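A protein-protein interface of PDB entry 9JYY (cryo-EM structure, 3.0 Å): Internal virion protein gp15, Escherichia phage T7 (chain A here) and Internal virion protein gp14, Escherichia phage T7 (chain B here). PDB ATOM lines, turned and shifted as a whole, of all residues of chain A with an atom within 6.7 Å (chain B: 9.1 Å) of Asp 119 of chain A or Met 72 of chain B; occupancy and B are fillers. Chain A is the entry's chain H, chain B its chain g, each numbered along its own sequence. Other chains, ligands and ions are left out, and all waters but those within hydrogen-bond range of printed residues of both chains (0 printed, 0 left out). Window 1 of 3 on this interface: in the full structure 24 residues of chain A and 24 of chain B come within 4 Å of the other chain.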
ATOM      1  N   ALA A 113      21.919   2.003  -6.235  1.00  0.00           N
ATOM      2  CA  ALA A 113      20.940   2.615  -7.121  1.00  0.00           C
ATOM      3  C   ALA A 113      20.069   3.604  -6.367  1.00  0.00           C
ATOM      4  O   ALA A 113      19.830   4.722  -6.833  1.00  0.00           O
ATOM      5  CB  ALA A 113      20.079   1.535  -7.769  1.00  0.00           C
ATOM      6  N   TYR A 114      19.592   3.211  -5.188  1.00  0.00           N
ATOM      7  CA  TYR A 114      18.692   4.085  -4.452  1.00  0.00           C
ATOM      8  C   TYR A 114      19.445   5.236  -3.810  1.00  0.00           C
ATOM      9  O   TYR A 114      19.347   6.379  -4.264  1.00  0.00           O
ATOM     10  CB  TYR A 114      17.956   3.292  -3.381  1.00  0.00           C
ATOM     11  CG  TYR A 114      16.693   2.625  -3.838  1.00  0.00           C
ATOM     12  CD1 TYR A 114      15.507   3.331  -3.914  1.00  0.00           C
ATOM     13  CD2 TYR A 114      16.685   1.288  -4.191  1.00  0.00           C
ATOM     14  CE1 TYR A 114      14.349   2.720  -4.318  1.00  0.00           C
ATOM     15  CE2 TYR A 114      15.534   0.670  -4.604  1.00  0.00           C
ATOM     16  CZ  TYR A 114      14.367   1.388  -4.668  1.00  0.00           C
ATOM     17  OH  TYR A 114      13.215   0.765  -5.083  1.00  0.00           O
ATOM     18  N   LEU A 115      20.287   4.936  -2.827  1.00  0.00           N
ATOM     19  CA  LEU A 115      20.708   5.947  -1.874  1.00  0.00           C
ATOM     20  C   LEU A 115      21.393   7.108  -2.562  1.00  0.00           C
ATOM     21  O   LEU A 115      20.741   8.112  -2.844  1.00  0.00           O
ATOM     22  CB  LEU A 115      21.667   5.335  -0.851  1.00  0.00           C
ATOM     23  CG  LEU A 115      22.517   6.311  -0.038  1.00  0.00           C
ATOM     24  CD1 LEU A 115      21.689   7.036   1.006  1.00  0.00           C
ATOM     25  CD2 LEU A 115      23.711   5.611   0.564  1.00  0.00           C
ATOM     26  N   VAL A 116      22.635   6.923  -2.998  1.00  0.00           N
ATOM     27  CA  VAL A 116      23.403   8.078  -3.439  1.00  0.00           C
ATOM     28  C   VAL A 116      22.718   8.704  -4.635  1.00  0.00           C
ATOM     29  O   VAL A 116      22.185   9.825  -4.564  1.00  0.00           O
ATOM     30  CB  VAL A 116      24.854   7.677  -3.766  1.00  0.00           C
ATOM     31  CG1 VAL A 116      25.689   8.915  -4.067  1.00  0.00           C
ATOM     32  CG2 VAL A 116      25.467   6.875  -2.627  1.00  0.00           C
ATOM     33  N   ASP A 117      22.617   7.925  -5.706  1.00  0.00           N
ATOM     34  CA  ASP A 117      22.114   8.431  -6.967  1.00  0.00           C
ATOM     35  C   ASP A 117      20.746   9.056  -6.789  1.00  0.00           C
ATOM     36  O   ASP A 117      20.585  10.267  -6.941  1.00  0.00           O
ATOM     37  CB  ASP A 117      22.058   7.296  -7.979  1.00  0.00           C
ATOM     38  CG  ASP A 117      23.418   6.721  -8.257  1.00  0.00           C
ATOM     39  OD1 ASP A 117      24.410   7.455  -8.086  1.00  0.00           O
ATOM     40  OD2 ASP A 117      23.498   5.542  -8.651  1.00  0.00           O
ATOM     41  N   ASP A 118      19.754   8.251  -6.417  1.00  0.00           N
ATOM     42  CA  ASP A 118      18.385   8.713  -6.528  1.00  0.00           C
ATOM     43  C   ASP A 118      18.001   9.672  -5.408  1.00  0.00           C
ATOM     44  O   ASP A 118      17.180  10.563  -5.632  1.00  0.00           O
ATOM     45  CB  ASP A 118      17.448   7.515  -6.587  1.00  0.00           C
ATOM     46  CG  ASP A 118      17.440   6.876  -7.951  1.00  0.00           C
ATOM     47  OD1 ASP A 118      17.807   7.571  -8.918  1.00  0.00           O
ATOM     48  OD2 ASP A 118      17.079   5.691  -8.068  1.00  0.00           O
ATOM     49  N   ASP A 119      18.554   9.542  -4.194  1.00  0.00           N
ATOM     50  CA  ASP A 119      18.122  10.495  -3.179  1.00  0.00           C
ATOM     51  C   ASP A 119      18.778  11.854  -3.395  1.00  0.00           C
ATOM     52  O   ASP A 119      18.129  12.894  -3.212  1.00  0.00           O
ATOM     53  CB  ASP A 119      18.350   9.948  -1.761  1.00  0.00           C
ATOM     54  CG  ASP A 119      19.759  10.174  -1.221  1.00  0.00           C
ATOM     55  OD1 ASP A 119      20.680  10.585  -1.957  1.00  0.00           O
ATOM     56  OD2 ASP A 119      19.947   9.933  -0.010  1.00  0.00           O
ATOM     57  N   VAL A 120      20.053  11.884  -3.816  1.00  0.00           N
ATOM     58  CA  VAL A 120      20.627  13.160  -4.222  1.00  0.00           C
ATOM     59  C   VAL A 120      19.892  13.690  -5.443  1.00  0.00           C
ATOM     60  O   VAL A 120      19.679  14.898  -5.589  1.00  0.00           O
ATOM     61  CB  VAL A 120      22.137  13.015  -4.480  1.00  0.00           C
ATOM     62  CG1 VAL A 120      22.678  14.229  -5.226  1.00  0.00           C
ATOM     63  CG2 VAL A 120      22.877  12.832  -3.165  1.00  0.00           C
ATOM     64  N   MET A 121      19.461  12.789  -6.323  1.00  0.00           N
ATOM     65  CA  MET A 121      18.719  13.187  -7.507  1.00  0.00           C
ATOM     66  C   MET A 121      17.414  13.864  -7.124  1.00  0.00           C
ATOM     67  O   MET A 121      17.049  14.897  -7.686  1.00  0.00           O
ATOM     68  CB  MET A 121      18.463  11.955  -8.370  1.00  0.00           C
ATOM     69  CG  MET A 121      17.976  12.267  -9.738  1.00  0.00           C
ATOM     70  SD  MET A 121      18.830  13.736 -10.295  1.00  0.00           S
ATOM     71  CE  MET A 121      18.151  13.885 -11.934  1.00  0.00           C
ATOM     72  N   GLN A 122      16.698  13.292  -6.154  1.00  0.00           N
ATOM     73  CA  GLN A 122      15.449  13.880  -5.685  1.00  0.00           C
ATOM     74  C   GLN A 122      15.686  15.220  -5.005  1.00  0.00           C
ATOM     75  O   GLN A 122      14.915  16.169  -5.201  1.00  0.00           O
ATOM     76  CB  GLN A 122      14.751  12.921  -4.730  1.00  0.00           C
ATOM     77  CG  GLN A 122      13.319  13.286  -4.463  1.00  0.00           C
ATOM     78  CD  GLN A 122      12.455  13.054  -5.661  1.00  0.00           C
ATOM     79  OE1 GLN A 122      12.219  13.967  -6.443  1.00  0.00           O
ATOM     80  NE2 GLN A 122      11.975  11.830  -5.821  1.00  0.00           N
ATOM     81  N   LYS A 123      16.739  15.316  -4.191  1.00  0.00           N
ATOM     82  CA  LYS A 123      17.057  16.591  -3.566  1.00  0.00           C
ATOM     83  C   LYS A 123      17.306  17.655  -4.624  1.00  0.00           C
ATOM     84  O   LYS A 123      16.827  18.789  -4.505  1.00  0.00           O
ATOM     85  CB  LYS A 123      18.279  16.442  -2.660  1.00  0.00           C
ATOM     86  CG  LYS A 123      18.495  17.591  -1.705  1.00  0.00           C
ATOM     87  CD  LYS A 123      17.231  17.864  -0.917  1.00  0.00           C
ATOM     88  CE  LYS A 123      17.320  19.168  -0.149  1.00  0.00           C
ATOM     89  NZ  LYS A 123      17.695  20.319  -1.009  1.00  0.00           N
ATOM     90  N   ILE A 124      18.039  17.302  -5.677  1.00  0.00           N
ATOM     91  CA  ILE A 124      18.325  18.262  -6.730  1.00  0.00           C
ATOM     92  C   ILE A 124      17.048  18.594  -7.502  1.00  0.00           C
ATOM     93  O   ILE A 124      16.843  19.740  -7.911  1.00  0.00           O
ATOM     94  CB  ILE A 124      19.445  17.710  -7.629  1.00  0.00           C
ATOM     95  CG1 ILE A 124      20.705  17.518  -6.804  1.00  0.00           C
ATOM     96  CG2 ILE A 124      19.859  18.715  -8.651  1.00  0.00           C
ATOM     97  CD1 ILE A 124      21.280  18.803  -6.289  1.00  0.00           C
ATOM     98  N   ARG A 139      20.934  12.335 -14.069  1.00  0.00           N
ATOM     99  CA  ARG A 139      20.675  11.044 -13.452  1.00  0.00           C
ATOM    100  C   ARG A 139      21.549   9.949 -14.047  1.00  0.00           C
ATOM    101  O   ARG A 139      22.082   9.117 -13.315  1.00  0.00           O
ATOM    102  CB  ARG A 139      19.195  10.701 -13.576  1.00  0.00           C
ATOM    103  CG  ARG A 139      18.856   9.265 -13.275  1.00  0.00           C
ATOM    104  CD  ARG A 139      17.364   9.063 -13.349  1.00  0.00           C
ATOM    105  NE  ARG A 139      16.984   7.659 -13.330  1.00  0.00           N
ATOM    106  CZ  ARG A 139      16.852   6.939 -12.227  1.00  0.00           C
ATOM    107  NH1 ARG A 139      17.267   7.387 -11.057  1.00  0.00           N
ATOM    108  NH2 ARG A 139      16.321   5.724 -12.308  1.00  0.00           N
ATOM    109  N   GLU A 173       9.943   1.570 -10.960  1.00  0.00           N
ATOM    110  CA  GLU A 173       9.102   2.425 -10.131  1.00  0.00           C
ATOM    111  C   GLU A 173       9.932   3.480  -9.412  1.00  0.00           C
ATOM    112  O   GLU A 173       9.397   4.508  -8.986  1.00  0.00           O
ATOM    113  CB  GLU A 173       8.245   1.586  -9.180  1.00  0.00           C
ATOM    114  CG  GLU A 173       8.938   0.721  -8.167  1.00  0.00           C
ATOM    115  CD  GLU A 173       9.227   1.453  -6.885  1.00  0.00           C
ATOM    116  OE1 GLU A 173       8.601   2.505  -6.650  1.00  0.00           O
ATOM    117  OE2 GLU A 173      10.042   0.955  -6.088  1.00  0.00           O
ATOM    118  N   ARG A 174      11.253   3.298  -9.354  1.00  0.00           N
ATOM    119  CA  ARG A 174      12.118   4.430  -9.036  1.00  0.00           C
ATOM    120  C   ARG A 174      11.985   5.516 -10.089  1.00  0.00           C
ATOM    121  O   ARG A 174      11.873   6.702  -9.761  1.00  0.00           O
ATOM    122  CB  ARG A 174      13.577   3.998  -8.935  1.00  0.00           C
ATOM    123  CG  ARG A 174      13.924   3.254  -7.678  1.00  0.00           C
ATOM    124  CD  ARG A 174      15.427   3.164  -7.516  1.00  0.00           C
ATOM    125  NE  ARG A 174      16.034   2.130  -8.340  1.00  0.00           N
ATOM    126  CZ  ARG A 174      16.996   2.350  -9.222  1.00  0.00           C
ATOM    127  NH1 ARG A 174      17.456   3.568  -9.452  1.00  0.00           N
ATOM    128  NH2 ARG A 174      17.513   1.322  -9.886  1.00  0.00           N
ATOM    129  N   ASN A 175      12.005   5.125 -11.363  1.00  0.00           N
ATOM    130  CA  ASN A 175      11.817   6.086 -12.440  1.00  0.00           C
ATOM    131  C   ASN A 175      10.444   6.726 -12.355  1.00  0.00           C
ATOM    132  O   ASN A 175      10.298   7.932 -12.574  1.00  0.00           O
ATOM    133  CB  ASN A 175      11.995   5.399 -13.791  1.00  0.00           C
ATOM    134  CG  ASN A 175      13.445   5.228 -14.168  1.00  0.00           C
ATOM    135  OD1 ASN A 175      14.316   5.928 -13.659  1.00  0.00           O
ATOM    136  ND2 ASN A 175      13.713   4.293 -15.067  1.00  0.00           N
ATOM    137  N   SER A 177       8.661   7.247  -9.649  1.00  0.00           N
ATOM    138  CA  SER A 177       8.682   8.216  -8.560  1.00  0.00           C
ATOM    139  C   SER A 177       9.448   9.474  -8.947  1.00  0.00           C
ATOM    140  O   SER A 177       8.982  10.591  -8.700  1.00  0.00           O
ATOM    141  CB  SER A 177       9.292   7.587  -7.311  1.00  0.00           C
ATOM    142  OG  SER A 177       9.605   8.582  -6.356  1.00  0.00           O
ATOM    143  N   LEU A 178      10.622   9.317  -9.560  1.00  0.00           N
ATOM    144  CA  LEU A 178      11.459  10.478  -9.853  1.00  0.00           C
ATOM    145  C   LEU A 178      10.835  11.363 -10.921  1.00  0.00           C
ATOM    146  O   LEU A 178      10.814  12.594 -10.790  1.00  0.00           O
ATOM    147  CB  LEU A 178      12.848  10.025 -10.288  1.00  0.00           C
ATOM    148  CG  LEU A 178      13.704   9.373  -9.206  1.00  0.00           C
ATOM    149  CD1 LEU A 178      14.663   8.445  -9.870  1.00  0.00           C
ATOM    150  CD2 LEU A 178      14.449  10.381  -8.358  1.00  0.00           C
ATOM    151  N   ALA B  28      25.376  19.001  -1.178  1.00  0.00           N
ATOM    152  CA  ALA B  28      25.636  17.705  -1.794  1.00  0.00           C
ATOM    153  C   ALA B  28      27.029  17.195  -1.448  1.00  0.00           C
ATOM    154  O   ALA B  28      27.215  16.001  -1.179  1.00  0.00           O
ATOM    155  CB  ALA B  28      25.454  17.798  -3.309  1.00  0.00           C
ATOM    156  N   THR B  31      26.894  15.888   2.051  1.00  0.00           N
ATOM    157  CA  THR B  31      26.245  14.579   2.100  1.00  0.00           C
ATOM    158  C   THR B  31      27.183  13.477   1.621  1.00  0.00           C
ATOM    159  O   THR B  31      27.237  12.391   2.218  1.00  0.00           O
ATOM    160  CB  THR B  31      24.969  14.585   1.263  1.00  0.00           C
ATOM    161  OG1 THR B  31      25.273  15.009  -0.071  1.00  0.00           O
ATOM    162  CG2 THR B  31      23.931  15.513   1.873  1.00  0.00           C
ATOM    163  N   ALA B  32      27.925  13.735   0.543  1.00  0.00           N
ATOM    164  CA  ALA B  32      28.891  12.752   0.064  1.00  0.00           C
ATOM    165  C   ALA B  32      29.973  12.497   1.104  1.00  0.00           C
ATOM    166  O   ALA B  32      30.378  11.350   1.325  1.00  0.00           O
ATOM    167  CB  ALA B  32      29.512  13.219  -1.251  1.00  0.00           C
ATOM    168  N   ARG B  35      28.545  10.265   3.819  1.00  0.00           N
ATOM    169  CA  ARG B  35      28.500   8.860   3.419  1.00  0.00           C
ATOM    170  C   ARG B  35      29.890   8.237   3.407  1.00  0.00           C
ATOM    171  O   ARG B  35      30.060   7.073   3.787  1.00  0.00           O
ATOM    172  CB  ARG B  35      27.834   8.715   2.056  1.00  0.00           C
ATOM    173  CG  ARG B  35      26.351   8.960   2.095  1.00  0.00           C
ATOM    174  CD  ARG B  35      25.817   9.248   0.725  1.00  0.00           C
ATOM    175  NE  ARG B  35      24.420   9.650   0.779  1.00  0.00           N
ATOM    176  CZ  ARG B  35      23.763  10.178  -0.241  1.00  0.00           C
ATOM    177  NH1 ARG B  35      24.352  10.386  -1.405  1.00  0.00           N
ATOM    178  NH2 ARG B  35      22.490  10.520  -0.084  1.00  0.00           N
ATOM    179  N   ALA B  65      22.187   4.782   9.310  1.00  0.00           N
ATOM    180  CA  ALA B  65      21.302   5.904   9.032  1.00  0.00           C
ATOM    181  C   ALA B  65      21.820   6.741   7.873  1.00  0.00           C
ATOM    182  O   ALA B  65      21.039   7.209   7.039  1.00  0.00           O
ATOM    183  CB  ALA B  65      21.132   6.764  10.284  1.00  0.00           C
ATOM    184  N   GLU B  66      23.136   6.948   7.803  1.00  0.00           N
ATOM    185  CA  GLU B  66      23.677   7.766   6.722  1.00  0.00           C
ATOM    186  C   GLU B  66      23.688   7.013   5.395  1.00  0.00           C
ATOM    187  O   GLU B  66      23.754   7.629   4.326  1.00  0.00           O
ATOM    188  CB  GLU B  66      25.071   8.263   7.093  1.00  0.00           C
ATOM    189  CG  GLU B  66      25.026   9.298   8.206  1.00  0.00           C
ATOM    190  CD  GLU B  66      26.388   9.834   8.588  1.00  0.00           C
ATOM    191  OE1 GLU B  66      27.401   9.305   8.090  1.00  0.00           O
ATOM    192  OE2 GLU B  66      26.438  10.784   9.398  1.00  0.00           O
ATOM    193  N   LEU B  67      23.632   5.680   5.439  1.00  0.00           N
ATOM    194  CA  LEU B  67      23.517   4.913   4.201  1.00  0.00           C
ATOM    195  C   LEU B  67      22.061   4.674   3.819  1.00  0.00           C
ATOM    196  O   LEU B  67      21.778   4.174   2.725  1.00  0.00           O
ATOM    197  CB  LEU B  67      24.265   3.585   4.314  1.00  0.00           C
ATOM    198  CG  LEU B  67      25.773   3.562   4.047  1.00  0.00           C
ATOM    199  CD1 LEU B  67      26.041   3.935   2.614  1.00  0.00           C
ATOM    200  CD2 LEU B  67      26.530   4.497   4.942  1.00  0.00           C
ATOM    201  N   THR B  68      21.126   5.007   4.704  1.00  0.00           N
ATOM    202  CA  THR B  68      19.722   4.989   4.318  1.00  0.00           C
ATOM    203  C   THR B  68      19.402   6.226   3.495  1.00  0.00           C
ATOM    204  O   THR B  68      19.952   7.306   3.726  1.00  0.00           O
ATOM    205  CB  THR B  68      18.814   4.936   5.546  1.00  0.00           C
ATOM    206  OG1 THR B  68      19.230   5.926   6.492  1.00  0.00           O
ATOM    207  CG2 THR B  68      18.863   3.570   6.195  1.00  0.00           C
ATOM    208  N   SER B  69      18.512   6.063   2.525  1.00  0.00           N
ATOM    209  CA  SER B  69      18.069   7.158   1.675  1.00  0.00           C
ATOM    210  C   SER B  69      16.930   7.884   2.372  1.00  0.00           C
ATOM    211  O   SER B  69      16.047   7.247   2.950  1.00  0.00           O
ATOM    212  CB  SER B  69      17.629   6.640   0.308  1.00  0.00           C
ATOM    213  OG  SER B  69      16.592   5.690   0.444  1.00  0.00           O
ATOM    214  N   GLN B  70      16.968   9.216   2.340  1.00  0.00           N
ATOM    215  CA  GLN B  70      15.895   9.996   2.947  1.00  0.00           C
ATOM    216  C   GLN B  70      14.779  10.276   1.951  1.00  0.00           C
ATOM    217  O   GLN B  70      13.606  10.013   2.238  1.00  0.00           O
ATOM    218  CB  GLN B  70      16.454  11.300   3.515  1.00  0.00           C
ATOM    219  CG  GLN B  70      17.825  11.166   4.156  1.00  0.00           C
ATOM    220  CD  GLN B  70      17.769  10.539   5.540  1.00  0.00           C
ATOM    221  OE1 GLN B  70      16.729  10.041   5.972  1.00  0.00           O
ATOM    222  NE2 GLN B  70      18.896  10.558   6.243  1.00  0.00           N
ATOM    223  N   ASN B  71      15.121  10.805   0.775  1.00  0.00           N
ATOM    224  CA  ASN B  71      14.095  11.152  -0.202  1.00  0.00           C
ATOM    225  C   ASN B  71      13.410   9.912  -0.764  1.00  0.00           C
ATOM    226  O   ASN B  71      12.179   9.870  -0.864  1.00  0.00           O
ATOM    227  CB  ASN B  71      14.701  11.983  -1.327  1.00  0.00           C
ATOM    228  CG  ASN B  71      15.218  13.324  -0.850  1.00  0.00           C
ATOM    229  OD1 ASN B  71      15.865  14.052  -1.599  1.00  0.00           O
ATOM    230  ND2 ASN B  71      14.919  13.666   0.394  1.00  0.00           N
ATOM    231  N   MET B  72      14.183   8.895  -1.136  1.00  0.00           N
ATOM    232  CA  MET B  72      13.637   7.678  -1.721  1.00  0.00           C
ATOM    233  C   MET B  72      13.375   6.605  -0.678  1.00  0.00           C
ATOM    234  O   MET B  72      13.360   5.417  -1.012  1.00  0.00           O
ATOM    235  CB  MET B  72      14.573   7.138  -2.801  1.00  0.00           C
ATOM    236  CG  MET B  72      15.234   8.201  -3.653  1.00  0.00           C
ATOM    237  SD  MET B  72      14.160   8.830  -4.948  1.00  0.00           S
ATOM    238  CE  MET B  72      13.688   7.308  -5.756  1.00  0.00           C
ATOM    239  N   GLN B  73      13.170   6.999   0.578  1.00  0.00           N
ATOM    240  CA  GLN B  73      12.972   6.016   1.637  1.00  0.00           C
ATOM    241  C   GLN B  73      11.679   5.235   1.435  1.00  0.00           C
ATOM    242  O   GLN B  73      11.640   4.017   1.640  1.00  0.00           O
ATOM    243  CB  GLN B  73      12.973   6.709   2.994  1.00  0.00           C
ATOM    244  CG  GLN B  73      12.789   5.762   4.147  1.00  0.00           C
ATOM    245  CD  GLN B  73      11.402   5.838   4.718  1.00  0.00           C
ATOM    246  OE1 GLN B  73      10.977   6.885   5.197  1.00  0.00           O
ATOM    247  NE2 GLN B  73      10.680   4.726   4.665  1.00  0.00           N
ATOM    248  N   LYS B  74      10.603   5.922   1.043  1.00  0.00           N
ATOM    249  CA  LYS B  74       9.331   5.238   0.833  1.00  0.00           C
ATOM    250  C   LYS B  74       9.452   4.214  -0.284  1.00  0.00           C
ATOM    251  O   LYS B  74       8.907   3.105  -0.196  1.00  0.00           O
ATOM    252  CB  LYS B  74       8.242   6.251   0.486  1.00  0.00           C
ATOM    253  CG  LYS B  74       7.973   7.287   1.554  1.00  0.00           C
ATOM    254  CD  LYS B  74       7.370   6.711   2.805  1.00  0.00           C
ATOM    255  CE  LYS B  74       7.069   7.835   3.777  1.00  0.00           C
ATOM    256  NZ  LYS B  74       6.514   7.339   5.055  1.00  0.00           N
ATOM    257  N   VAL B  75      10.158   4.582  -1.351  1.00  0.00           N
ATOM    258  CA  VAL B  75      10.335   3.687  -2.487  1.00  0.00           C
ATOM    259  C   VAL B  75      11.201   2.499  -2.096  1.00  0.00           C
ATOM    260  O   VAL B  75      10.912   1.356  -2.468  1.00  0.00           O
ATOM    261  CB  VAL B  75      10.920   4.466  -3.674  1.00  0.00           C
ATOM    262  CG1 VAL B  75      11.065   3.572  -4.868  1.00  0.00           C
ATOM    263  CG2 VAL B  75      10.029   5.648  -4.005  1.00  0.00           C
ATOM    264  N   GLN B  76      12.270   2.745  -1.332  1.00  0.00           N
ATOM    265  CA  GLN B  76      13.047   1.647  -0.763  1.00  0.00           C
ATOM    266  C   GLN B  76      12.166   0.696   0.030  1.00  0.00           C
ATOM    267  O   GLN B  76      12.262  -0.523  -0.128  1.00  0.00           O
ATOM    268  CB  GLN B  76      14.144   2.185   0.151  1.00  0.00           C
ATOM    269  CG  GLN B  76      15.366   2.749  -0.512  1.00  0.00           C
ATOM    270  CD  GLN B  76      16.470   1.727  -0.588  1.00  0.00           C
ATOM    271  OE1 GLN B  76      16.210   0.530  -0.674  1.00  0.00           O
ATOM    272  NE2 GLN B  76      17.709   2.183  -0.498  1.00  0.00           N
ATOM    273  N   ALA B  77      11.322   1.236   0.909  1.00  0.00           N
ATOM    274  CA  ALA B  77      10.510   0.390   1.772  1.00  0.00           C
ATOM    275  C   ALA B  77       9.541  -0.458   0.966  1.00  0.00           C
ATOM    276  O   ALA B  77       9.417  -1.667   1.202  1.00  0.00           O
ATOM    277  CB  ALA B  77       9.751   1.250   2.780  1.00  0.00           C
ATOM    278  N   ILE B  78       8.845   0.152   0.008  1.00  0.00           N
ATOM    279  CA  ILE B  78       7.864  -0.606  -0.761  1.00  0.00           C
ATOM    280  C   ILE B  78       8.560  -1.636  -1.642  1.00  0.00           C
ATOM    281  O   ILE B  78       8.071  -2.760  -1.810  1.00  0.00           O
ATOM    282  CB  ILE B  78       6.953   0.340  -1.565  1.00  0.00           C
ATOM    283  CG1 ILE B  78       5.809  -0.442  -2.205  1.00  0.00           C
ATOM    284  CG2 ILE B  78       7.733   1.105  -2.609  1.00  0.00           C
ATOM    285  CD1 ILE B  78       4.725   0.436  -2.783  1.00  0.00           C
ATOM    286  N   GLY B  79       9.727  -1.289  -2.189  1.00  0.00           N
ATOM    287  CA  GLY B  79      10.469  -2.251  -2.985  1.00  0.00           C
ATOM    288  C   GLY B  79      10.982  -3.416  -2.164  1.00  0.00           C
ATOM    289  O   GLY B  79      10.954  -4.563  -2.613  1.00  0.00           O
ATOM    290  N   SER B  80      11.463  -3.140  -0.952  1.00  0.00           N
ATOM    291  CA  SER B  80      11.923  -4.214  -0.080  1.00  0.00           C
ATOM    292  C   SER B  80      10.772  -5.121   0.315  1.00  0.00           C
ATOM    293  O   SER B  80      10.923  -6.349   0.352  1.00  0.00           O
ATOM    294  CB  SER B  80      12.593  -3.633   1.165  1.00  0.00           C
ATOM    295  OG  SER B  80      13.751  -2.893   0.824  1.00  0.00           O
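NH2 of Arg 35 of chain B lies within salt-bridge range of OD1 of Asp 119 of chain A.
The side-chain amide oxygen (OD1) of Asn 71 of chain B lies close to the backbone carbonyl oxygen (O) of Asp 119 of chain A.
OD1 of Asn 71 of chain B lies within hydrogen-bond range of N of Lys 123 of chain A (3.0 Å).
The side-chain sulfur (SD) of Met 72 of chain B sits close to the backbone carbonyl oxygen (O) of Asp 118 of chain A (3.5 Å).
The backbone carbonyl oxygen (O) of Gln 76 of chain B lies within hydrogen-bond range of the side-chain hydroxyl (OG) of Ser 80 of chain B (3.0 Å).
The backbone carbonyl oxygen (O) of Tyr 114 of chain A lies within hydrogen-bond range of the backbone NH (N) of Asp 119 of chain A, at 3.3 Å.
OE2 of Glu 173 of chain A is in hydrogen-bond range of OH of Tyr 114 of chain A, at 3.3 Å.
O of Leu 115 of chain A sits close to OD1 of Asp 119 of chain A, 2.6 Å away.
OD2 of Asp 118 of chain A lies within salt-bridge range of NH1 of Arg 139 of chain A (3.4 Å).
The guanidinium group (NH1) of Arg 174 of chain A is in salt-bridge range of the side-chain carboxylate (OD2) of Asp 118 of chain A (2.6 Å).
Among the printed residues, pairs that only touch across the chains: Glu 173 of chain A with Val 75 of chain B (3.1 Å), Tyr 114 of chain A with Gln 76 of chain B (3.1 Å), Val 116 of chain A with Arg 35 of chain B (3.2 Å), Leu 115 of chain A with Leu 67 of chain B (3.2 Å), Leu 115 of chain A with Thr 68 of chain B (3.2 Å), Val 120 of chain A with Arg 35 of chain B (3.4 Å), Tyr 114 of chain A with Val 75 of chain B (3.4 Å), Gln 122 of chain A with Asn 71 of chain B (3.5 Å), Asp 119 of chain A with Met 72 of chain B (3.6 Å), Leu 115 of chain A with Ser 69 of chain B (3.7 Å), Leu 115 of chain A with Arg 35 of chain B (3.7 Å), Asp 119 of chain A with Ser 69 of chain B (3.8 Å), Leu 178 of chain A with Met 72 of chain B (3.8 Å), Ser 177 of chain A with Val 75 of chain B (3.8 Å), Gln 122 of chain A with Met 72 of chain B (3.8 Å), Asp 119 of chain A with Gln 70 of chain B (3.9 Å) and Leu 115 of chain A with Glu 66 of chain B (3.95 Å).
Of the printed residues of chain B, Leu 115 of chain A touches Arg 35 (3.7 Å), Glu 66 (3.95 Å), Leu 67 (3.2 Å), Thr 68 (3.2 Å) and Ser 69 (3.7 Å).
Asp 119 of chain A touches five residues of chain B.
Val 120 of chain A touches just one residue of chain B: Arg 35.
Of the printed residues of chain B, Lys 123 of chain A touches Asn 71.
Ala 32 of chain B touches none of the printed residues of chain A.
Printed residues of chain A within 4 Å of Leu 67 of chain B: Leu 115.
Printed residues of chain A within 4 Å of Gln 70 of chain B: Asp 119 (3.9 Å).
Lys 74 of chain B touches none of the printed residues of chain A.
The nearest residue of chain A that does not touch Met 72 of chain B is Tyr 114 of chain A (4.1 Å).
Of the 20 printed residues of chain B, 10 touch a printed residue of chain A.
Hydrophobic or aromatic side chains of chain B within 4 Å of the printed part of chain A: Leu 67, Met 72 and Val 75.
Printed residues of chain A that touch a printed residue of chain B: Tyr 114, Leu 115, Val 116, Asp 118, Asp 119, Val 120, Gln 122, Lys 123, Glu 173, Ser 177 and Leu 178.
Along chain A the printed residues that touch a printed residue of chain B span positions 114 to 178.
Among the printed residues, Asp or Glu carboxylates within 4 Å of a Lys or Arg side-chain nitrogen of the other chain: Asp 119 of chain A with Arg 35 of chain B (2.6 Å).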
